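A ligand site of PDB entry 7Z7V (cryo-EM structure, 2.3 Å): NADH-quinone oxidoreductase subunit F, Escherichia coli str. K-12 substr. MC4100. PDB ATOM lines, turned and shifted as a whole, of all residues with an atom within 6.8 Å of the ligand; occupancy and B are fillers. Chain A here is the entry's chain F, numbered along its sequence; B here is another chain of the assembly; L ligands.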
ATOM      1  N   ILE A 179      32.640  14.568 -18.859  1.00  0.00           N
ATOM      2  CA  ILE A 179      32.656  15.875 -18.205  1.00  0.00           C
ATOM      3  C   ILE A 179      33.587  16.855 -18.912  1.00  0.00           C
ATOM      4  O   ILE A 179      33.451  18.065 -18.743  1.00  0.00           O
ATOM      5  CB  ILE A 179      33.043  15.704 -16.723  1.00  0.00           C
ATOM      6  CG1 ILE A 179      32.675  16.948 -15.895  1.00  0.00           C
ATOM      7  CG2 ILE A 179      34.513  15.349 -16.561  1.00  0.00           C
ATOM      8  CD1 ILE A 179      31.315  17.512 -16.188  1.00  0.00           C
ATOM      9  N   GLU A 182      32.006  19.886 -20.725  1.00  0.00           N
ATOM     10  CA  GLU A 182      31.673  21.089 -19.978  1.00  0.00           C
ATOM     11  C   GLU A 182      32.795  22.102 -20.150  1.00  0.00           C
ATOM     12  O   GLU A 182      33.968  21.764 -20.019  1.00  0.00           O
ATOM     13  CB  GLU A 182      31.476  20.760 -18.495  1.00  0.00           C
ATOM     14  CG  GLU A 182      30.521  21.688 -17.768  1.00  0.00           C
ATOM     15  CD  GLU A 182      31.204  22.905 -17.188  1.00  0.00           C
ATOM     16  OE1 GLU A 182      32.452  22.940 -17.163  1.00  0.00           O
ATOM     17  OE2 GLU A 182      30.491  23.834 -16.770  1.00  0.00           O
ATOM     18  N   ALA A 195      39.676  17.137 -15.262  1.00  0.00           N
ATOM     19  CA  ALA A 195      38.616  17.939 -15.850  1.00  0.00           C
ATOM     20  C   ALA A 195      37.474  18.196 -14.865  1.00  0.00           C
ATOM     21  O   ALA A 195      36.337  17.803 -15.065  1.00  0.00           O
ATOM     22  CB  ALA A 195      38.104  17.284 -17.131  1.00  0.00           C
ATOM     23  N   ASN A 196      37.814  18.853 -13.774  1.00  0.00           N
ATOM     24  CA  ASN A 196      36.763  19.412 -12.953  1.00  0.00           C
ATOM     25  C   ASN A 196      36.301  20.737 -13.559  1.00  0.00           C
ATOM     26  O   ASN A 196      37.122  21.485 -14.102  1.00  0.00           O
ATOM     27  CB  ASN A 196      37.234  19.648 -11.521  1.00  0.00           C
ATOM     28  CG  ASN A 196      37.779  18.393 -10.870  1.00  0.00           C
ATOM     29  OD1 ASN A 196      38.964  18.288 -10.595  1.00  0.00           O
ATOM     30  ND2 ASN A 196      36.900  17.431 -10.631  1.00  0.00           N
ATOM     31  N   PRO A 197      35.016  21.047 -13.500  1.00  0.00           N
ATOM     32  CA  PRO A 197      34.559  22.353 -13.954  1.00  0.00           C
ATOM     33  C   PRO A 197      34.932  23.441 -12.951  1.00  0.00           C
ATOM     34  O   PRO A 197      35.396  23.177 -11.841  1.00  0.00           O
ATOM     35  CB  PRO A 197      33.040  22.195 -14.063  1.00  0.00           C
ATOM     36  CG  PRO A 197      32.715  21.039 -13.226  1.00  0.00           C
ATOM     37  CD  PRO A 197      33.901  20.142 -13.173  1.00  0.00           C
ATOM     38  N   PHE A 346      25.533   8.336 -16.131  1.00  0.00           N
ATOM     39  CA  PHE A 346      25.711   9.644 -15.505  1.00  0.00           C
ATOM     40  C   PHE A 346      26.495   9.539 -14.194  1.00  0.00           C
ATOM     41  O   PHE A 346      27.295  10.421 -13.887  1.00  0.00           O
ATOM     42  CB  PHE A 346      24.343  10.286 -15.267  1.00  0.00           C
ATOM     43  CG  PHE A 346      23.785  10.967 -16.481  1.00  0.00           C
ATOM     44  CD1 PHE A 346      24.480  11.969 -17.123  1.00  0.00           C
ATOM     45  CD2 PHE A 346      22.546  10.592 -16.980  1.00  0.00           C
ATOM     46  CE1 PHE A 346      23.965  12.586 -18.242  1.00  0.00           C
ATOM     47  CE2 PHE A 346      22.018  11.205 -18.102  1.00  0.00           C
ATOM     48  CZ  PHE A 346      22.734  12.204 -18.732  1.00  0.00           C
ATOM     49  N   GLU A 349      30.184   8.877 -14.954  1.00  0.00           N
ATOM     50  CA  GLU A 349      30.808  10.016 -15.613  1.00  0.00           C
ATOM     51  C   GLU A 349      30.852  11.243 -14.727  1.00  0.00           C
ATOM     52  O   GLU A 349      31.196  12.335 -15.196  1.00  0.00           O
ATOM     53  CB  GLU A 349      30.080  10.345 -16.916  1.00  0.00           C
ATOM     54  CG  GLU A 349      30.414   9.385 -18.046  1.00  0.00           C
ATOM     55  CD  GLU A 349      31.908   9.193 -18.228  1.00  0.00           C
ATOM     56  OE1 GLU A 349      32.623  10.181 -18.459  1.00  0.00           O
ATOM     57  OE2 GLU A 349      32.365   8.033 -18.120  1.00  0.00           O
ATOM     58  N   SER A 350      30.497  11.094 -13.457  1.00  0.00           N
ATOM     59  CA  SER A 350      30.694  12.157 -12.472  1.00  0.00           C
ATOM     60  C   SER A 350      32.175  12.475 -12.360  1.00  0.00           C
ATOM     61  O   SER A 350      33.027  11.584 -12.360  1.00  0.00           O
ATOM     62  CB  SER A 350      30.161  11.702 -11.117  1.00  0.00           C
ATOM     63  OG  SER A 350      30.323  12.704 -10.137  1.00  0.00           O
ATOM     64  N   CYS A 351      32.491  13.769 -12.294  1.00  0.00           N
ATOM     65  CA  CYS A 351      33.881  14.137 -12.095  1.00  0.00           C
ATOM     66  C   CYS A 351      34.318  13.993 -10.641  1.00  0.00           C
ATOM     67  O   CYS A 351      35.524  14.029 -10.369  1.00  0.00           O
ATOM     68  CB  CYS A 351      34.127  15.557 -12.595  1.00  0.00           C
ATOM     69  SG  CYS A 351      33.848  16.828 -11.389  1.00  0.00           S
ATOM     70  N   GLY A 352      33.378  13.811  -9.722  1.00  0.00           N
ATOM     71  CA  GLY A 352      33.703  13.575  -8.326  1.00  0.00           C
ATOM     72  C   GLY A 352      33.961  14.798  -7.498  1.00  0.00           C
ATOM     73  O   GLY A 352      34.363  14.667  -6.335  1.00  0.00           O
ATOM     74  N   TRP A 353      33.749  15.994  -8.052  1.00  0.00           N
ATOM     75  CA  TRP A 353      34.055  17.219  -7.315  1.00  0.00           C
ATOM     76  C   TRP A 353      33.051  17.481  -6.209  1.00  0.00           C
ATOM     77  O   TRP A 353      33.438  17.842  -5.089  1.00  0.00           O
ATOM     78  CB  TRP A 353      34.115  18.401  -8.280  1.00  0.00           C
ATOM     79  CG  TRP A 353      34.267  19.746  -7.650  1.00  0.00           C
ATOM     80  CD1 TRP A 353      33.329  20.739  -7.620  1.00  0.00           C
ATOM     81  CD2 TRP A 353      35.429  20.269  -7.008  1.00  0.00           C
ATOM     82  NE1 TRP A 353      33.837  21.844  -6.978  1.00  0.00           N
ATOM     83  CE2 TRP A 353      35.120  21.575  -6.595  1.00  0.00           C
ATOM     84  CE3 TRP A 353      36.698  19.753  -6.737  1.00  0.00           C
ATOM     85  CZ2 TRP A 353      36.035  22.373  -5.923  1.00  0.00           C
ATOM     86  CZ3 TRP A 353      37.600  20.547  -6.068  1.00  0.00           C
ATOM     87  CH2 TRP A 353      37.272  21.846  -5.666  1.00  0.00           C
ATOM     88  N   CYS A 354      31.767  17.331  -6.490  1.00  0.00           N
ATOM     89  CA  CYS A 354      30.743  17.801  -5.568  1.00  0.00           C
ATOM     90  C   CYS A 354      29.828  16.677  -5.114  1.00  0.00           C
ATOM     91  O   CYS A 354      29.518  15.759  -5.885  1.00  0.00           O
ATOM     92  CB  CYS A 354      29.957  18.977  -6.177  1.00  0.00           C
ATOM     93  SG  CYS A 354      28.646  18.634  -7.333  1.00  0.00           S
ATOM     94  N   THR A 355      29.426  16.758  -3.848  1.00  0.00           N
ATOM     95  CA  THR A 355      28.751  15.668  -3.150  1.00  0.00           C
ATOM     96  C   THR A 355      27.446  15.174  -3.788  1.00  0.00           C
ATOM     97  O   THR A 355      27.294  13.957  -3.922  1.00  0.00           O
ATOM     98  CB  THR A 355      28.521  16.062  -1.685  1.00  0.00           C
ATOM     99  OG1 THR A 355      29.770  16.370  -1.070  1.00  0.00           O
ATOM    100  CG2 THR A 355      27.842  14.943  -0.925  1.00  0.00           C
ATOM    101  N   PRO A 356      26.462  16.029  -4.160  1.00  0.00           N
ATOM    102  CA  PRO A 356      25.172  15.484  -4.616  1.00  0.00           C
ATOM    103  C   PRO A 356      25.273  14.597  -5.837  1.00  0.00           C
ATOM    104  O   PRO A 356      24.744  13.492  -5.815  1.00  0.00           O
ATOM    105  CB  PRO A 356      24.346  16.738  -4.909  1.00  0.00           C
ATOM    106  CG  PRO A 356      24.958  17.777  -4.099  1.00  0.00           C
ATOM    107  CD  PRO A 356      26.403  17.502  -4.220  1.00  0.00           C
ATOM    108  N   CYS A 357      26.035  15.001  -6.848  1.00  0.00           N
ATOM    109  CA  CYS A 357      26.191  14.149  -8.017  1.00  0.00           C
ATOM    110  C   CYS A 357      27.013  12.911  -7.691  1.00  0.00           C
ATOM    111  O   CYS A 357      26.519  11.778  -7.840  1.00  0.00           O
ATOM    112  CB  CYS A 357      26.816  14.969  -9.141  1.00  0.00           C
ATOM    113  SG  CYS A 357      27.715  14.162 -10.468  1.00  0.00           S
ATOM    114  N   ARG A 358      28.188  13.107  -7.075  1.00  0.00           N
ATOM    115  CA  ARG A 358      29.156  12.039  -6.851  1.00  0.00           C
ATOM    116  C   ARG A 358      28.614  10.954  -5.930  1.00  0.00           C
ATOM    117  O   ARG A 358      28.892   9.763  -6.118  1.00  0.00           O
ATOM    118  CB  ARG A 358      30.450  12.629  -6.290  1.00  0.00           C
ATOM    119  CG  ARG A 358      31.466  11.611  -5.781  1.00  0.00           C
ATOM    120  CD  ARG A 358      32.575  12.254  -4.965  1.00  0.00           C
ATOM    121  NE  ARG A 358      32.138  12.556  -3.609  1.00  0.00           N
ATOM    122  CZ  ARG A 358      32.045  13.782  -3.116  1.00  0.00           C
ATOM    123  NH1 ARG A 358      32.379  14.842  -3.826  1.00  0.00           N
ATOM    124  NH2 ARG A 358      31.607  13.954  -1.873  1.00  0.00           N
ATOM    125  N   LEU A 361      24.006  10.193  -7.350  1.00  0.00           N
ATOM    126  CA  LEU A 361      23.785   9.402  -8.553  1.00  0.00           C
ATOM    127  C   LEU A 361      24.040   7.909  -8.361  1.00  0.00           C
ATOM    128  O   LEU A 361      23.223   7.118  -8.863  1.00  0.00           O
ATOM    129  CB  LEU A 361      24.610   9.988  -9.717  1.00  0.00           C
ATOM    130  CG  LEU A 361      24.116  11.330 -10.260  1.00  0.00           C
ATOM    131  CD1 LEU A 361      24.989  11.805 -11.402  1.00  0.00           C
ATOM    132  CD2 LEU A 361      22.678  11.226 -10.696  1.00  0.00           C
ATOM    133  N   THR A 396      24.084  21.467  -7.337  1.00  0.00           N
ATOM    134  CA  THR A 396      25.367  20.870  -7.661  1.00  0.00           C
ATOM    135  C   THR A 396      26.292  21.925  -8.256  1.00  0.00           C
ATOM    136  O   THR A 396      25.876  23.033  -8.603  1.00  0.00           O
ATOM    137  CB  THR A 396      25.194  19.695  -8.609  1.00  0.00           C
ATOM    138  OG1 THR A 396      24.733  20.175  -9.885  1.00  0.00           O
ATOM    139  CG2 THR A 396      24.188  18.717  -8.053  1.00  0.00           C
ATOM    140  N   PHE A 397      27.568  21.558  -8.374  1.00  0.00           N
ATOM    141  CA  PHE A 397      28.570  22.518  -8.811  1.00  0.00           C
ATOM    142  C   PHE A 397      28.443  22.833 -10.296  1.00  0.00           C
ATOM    143  O   PHE A 397      28.659  23.979 -10.717  1.00  0.00           O
ATOM    144  CB  PHE A 397      29.962  22.002  -8.480  1.00  0.00           C
ATOM    145  CG  PHE A 397      31.049  23.013  -8.668  1.00  0.00           C
ATOM    146  CD1 PHE A 397      31.302  23.970  -7.704  1.00  0.00           C
ATOM    147  CD2 PHE A 397      31.834  23.005  -9.816  1.00  0.00           C
ATOM    148  CE1 PHE A 397      32.305  24.893  -7.869  1.00  0.00           C
ATOM    149  CE2 PHE A 397      32.837  23.928  -9.982  1.00  0.00           C
ATOM    150  CZ  PHE A 397      33.070  24.871  -9.012  1.00  0.00           C
ATOM    151  N   CYS A 398      28.112  21.838 -11.112  1.00  0.00           N
ATOM    152  CA  CYS A 398      27.912  22.053 -12.541  1.00  0.00           C
ATOM    153  C   CYS A 398      26.606  21.384 -12.967  1.00  0.00           C
ATOM    154  O   CYS A 398      25.900  20.784 -12.154  1.00  0.00           O
ATOM    155  CB  CYS A 398      29.108  21.531 -13.354  1.00  0.00           C
ATOM    156  SG  CYS A 398      28.979  19.831 -13.908  1.00  0.00           S
ATOM    157  N   ALA A 399      26.290  21.486 -14.259  1.00  0.00           N
ATOM    158  CA  ALA A 399      24.995  21.062 -14.780  1.00  0.00           C
ATOM    159  C   ALA A 399      24.953  19.599 -15.202  1.00  0.00           C
ATOM    160  O   ALA A 399      24.012  19.194 -15.875  1.00  0.00           O
ATOM    161  CB  ALA A 399      24.597  21.946 -15.956  1.00  0.00           C
ATOM    162  N   HIS A 400      25.964  18.813 -14.834  1.00  0.00           N
ATOM    163  CA  HIS A 400      25.945  17.386 -15.161  1.00  0.00           C
ATOM    164  C   HIS A 400      24.809  16.662 -14.455  1.00  0.00           C
ATOM    165  O   HIS A 400      24.061  15.894 -15.070  1.00  0.00           O
ATOM    166  CB  HIS A 400      27.294  16.760 -14.802  1.00  0.00           C
ATOM    167  CG  HIS A 400      27.293  15.264 -14.783  1.00  0.00           C
ATOM    168  ND1 HIS A 400      27.532  14.506 -15.902  1.00  0.00           N
ATOM    169  CD2 HIS A 400      27.102  14.386 -13.772  1.00  0.00           C
ATOM    170  CE1 HIS A 400      27.478  13.229 -15.583  1.00  0.00           C
ATOM    171  NE2 HIS A 400      27.213  13.125 -14.299  1.00  0.00           N
ATOM    172  N   ALA A 401      24.647  16.909 -13.164  1.00  0.00           N
ATOM    173  CA  ALA A 401      23.634  16.235 -12.356  1.00  0.00           C
ATOM    174  C   ALA A 401      22.187  16.681 -12.615  1.00  0.00           C
ATOM    175  O   ALA A 401      21.288  15.826 -12.538  1.00  0.00           O
ATOM    176  CB  ALA A 401      23.965  16.376 -10.877  1.00  0.00           C
ATOM    177  N   PRO A 402      21.880  17.972 -12.861  1.00  0.00           N
ATOM    178  CA  PRO A 402      20.509  18.289 -13.317  1.00  0.00           C
ATOM    179  C   PRO A 402      20.116  17.587 -14.606  1.00  0.00           C
ATOM    180  O   PRO A 402      18.977  17.095 -14.732  1.00  0.00           O
ATOM    181  CB  PRO A 402      20.540  19.812 -13.488  1.00  0.00           C
ATOM    182  CG  PRO A 402      21.536  20.257 -12.543  1.00  0.00           C
ATOM    183  CD  PRO A 402      22.597  19.210 -12.519  1.00  0.00           C
ATOM    184  N   ALA B  44      32.790  22.854  -3.099  1.00  0.00           N
ATOM    185  CA  ALA B  44      32.811  21.441  -3.455  1.00  0.00           C
ATOM    186  C   ALA B  44      31.760  20.635  -2.686  1.00  0.00           C
ATOM    187  O   ALA B  44      30.901  19.998  -3.303  1.00  0.00           O
ATOM    188  CB  ALA B  44      34.197  20.851  -3.217  1.00  0.00           C
ATOM    189  N   ARG B  46      29.100  21.172  -1.032  1.00  0.00           N
ATOM    190  CA  ARG B  46      27.704  21.612  -1.123  1.00  0.00           C
ATOM    191  C   ARG B  46      26.968  21.547   0.218  1.00  0.00           C
ATOM    192  O   ARG B  46      25.744  21.497   0.245  1.00  0.00           O
ATOM    193  CB  ARG B  46      26.936  20.846  -2.205  1.00  0.00           C
ATOM    194  CG  ARG B  46      27.661  20.722  -3.533  1.00  0.00           C
ATOM    195  CD  ARG B  46      28.109  22.056  -4.067  1.00  0.00           C
ATOM    196  NE  ARG B  46      27.041  22.791  -4.713  1.00  0.00           N
ATOM    197  CZ  ARG B  46      27.220  23.919  -5.375  1.00  0.00           C
ATOM    198  NH1 ARG B  46      28.428  24.443  -5.524  1.00  0.00           N
ATOM    199  NH2 ARG B  46      26.169  24.536  -5.903  1.00  0.00           N
ATOM    200  N   HIS B 176      34.652  10.043 -10.246  1.00  0.00           N
ATOM    201  CA  HIS B 176      33.331   9.865  -9.634  1.00  0.00           C
ATOM    202  C   HIS B 176      33.404   9.571  -8.135  1.00  0.00           C
ATOM    203  O   HIS B 176      34.081  10.295  -7.399  1.00  0.00           O
ATOM    204  CB  HIS B 176      32.506   8.790 -10.373  1.00  0.00           C
ATOM    205  CG  HIS B 176      33.280   7.568 -10.760  1.00  0.00           C
ATOM    206  ND1 HIS B 176      33.343   6.441  -9.966  1.00  0.00           N
ATOM    207  CD2 HIS B 176      34.022   7.290 -11.847  1.00  0.00           C
ATOM    208  CE1 HIS B 176      34.092   5.528 -10.546  1.00  0.00           C
ATOM    209  NE2 HIS B 176      34.515   6.021 -11.698  1.00  0.00           N
HETATM  210 FE1  LIG L   1      29.523  18.034  -9.396  1.00  0.00          FE
HETATM  211 FE2  LIG L   1      29.073  15.987 -10.930  1.00  0.00          FE
HETATM  212 FE3  LIG L   1      29.506  18.423 -12.132  1.00  0.00          FE
HETATM  213 FE4  LIG L   1      31.555  17.128 -11.058  1.00  0.00          FE
HETATM  214  S1  LIG L   1      30.310  16.375 -12.832  1.00  0.00           S
HETATM  215  S2  LIG L   1      31.003  19.317 -10.613  1.00  0.00           S
HETATM  216  S3  LIG L   1      30.646  16.030  -9.252  1.00  0.00           S
HETATM  217  S4  LIG L   1      27.728  17.847 -10.811  1.00  0.00           S
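The side-chain hydroxyl (OG) of Ser 350 sits close to the backbone NH (N) of Gly 352, at 3.3 Å. The backbone carbonyl oxygen of Trp 353 is in hydrogen-bond range of the guanidinium group of Arg 358 (3.4 Å). The backbone NH of Phe 397 sits close to the side-chain sulfur of Cys 354 (3.3 Å). OG1 of Thr 396 lies within hydrogen-bond range of O of Cys 398 (2.6 Å). The side-chain sulfur of Cys 357 sits close to the side-chain hydroxyl of Ser 350 (3.0 Å). The backbone carbonyl oxygen of Thr 396 lies within hydrogen-bond range of the guanidinium group of Arg 46 of chain B, at 3.1 Å. ND2 of Asn 196 sits close to SG of Cys 351 (3.2 Å). N of His 400 lies close to SG of Cys 398, 3.3 Å away.
SG of Cys 354 binds FE1 of the ligand (2.3 Å). S3 of the ligand lies close to OG of Ser 350 (3.5 Å). The side-chain sulfur (SG) of Cys 351 binds an iron atom (FE4) of the ligand, 2.3 Å away. The backbone NH (N) of Cys 351 lies close to a sulfur (S1) of the ligand, at 3.4 Å. The side-chain sulfur of Cys 357 is bound to an iron atom (FE2) of the ligand, 2.3 Å away. A sulfur (S3) of the ligand lies close to the backbone NH (N) of Trp 353 (3.3 Å). FE3 of the ligand is bound by SG of Cys 398, 2.3 Å away. S3 of the ligand lies close to N of Gly 352 (3.6 Å). N of Cys 354 lies close to S3 of the ligand (3.3 Å).
CD1 of Ile 179 touches S1 of the ligand, 3.7 Å away. Pro 197 touches the ligand. Thr 396 touches the ligand. CB of Phe 397 touches S2 of the ligand (3.6 Å). His 400 touches the ligand (CB to S1, 3.6 Å). Ala 401 touches the ligand. Hydrophobic or aromatic side chains within 4 Å of the ligand: Ile 179, Pro 197, Trp 353, Phe 397 and His 400. Of the 27 residues printed, 13 come within 4 Å of the ligand.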
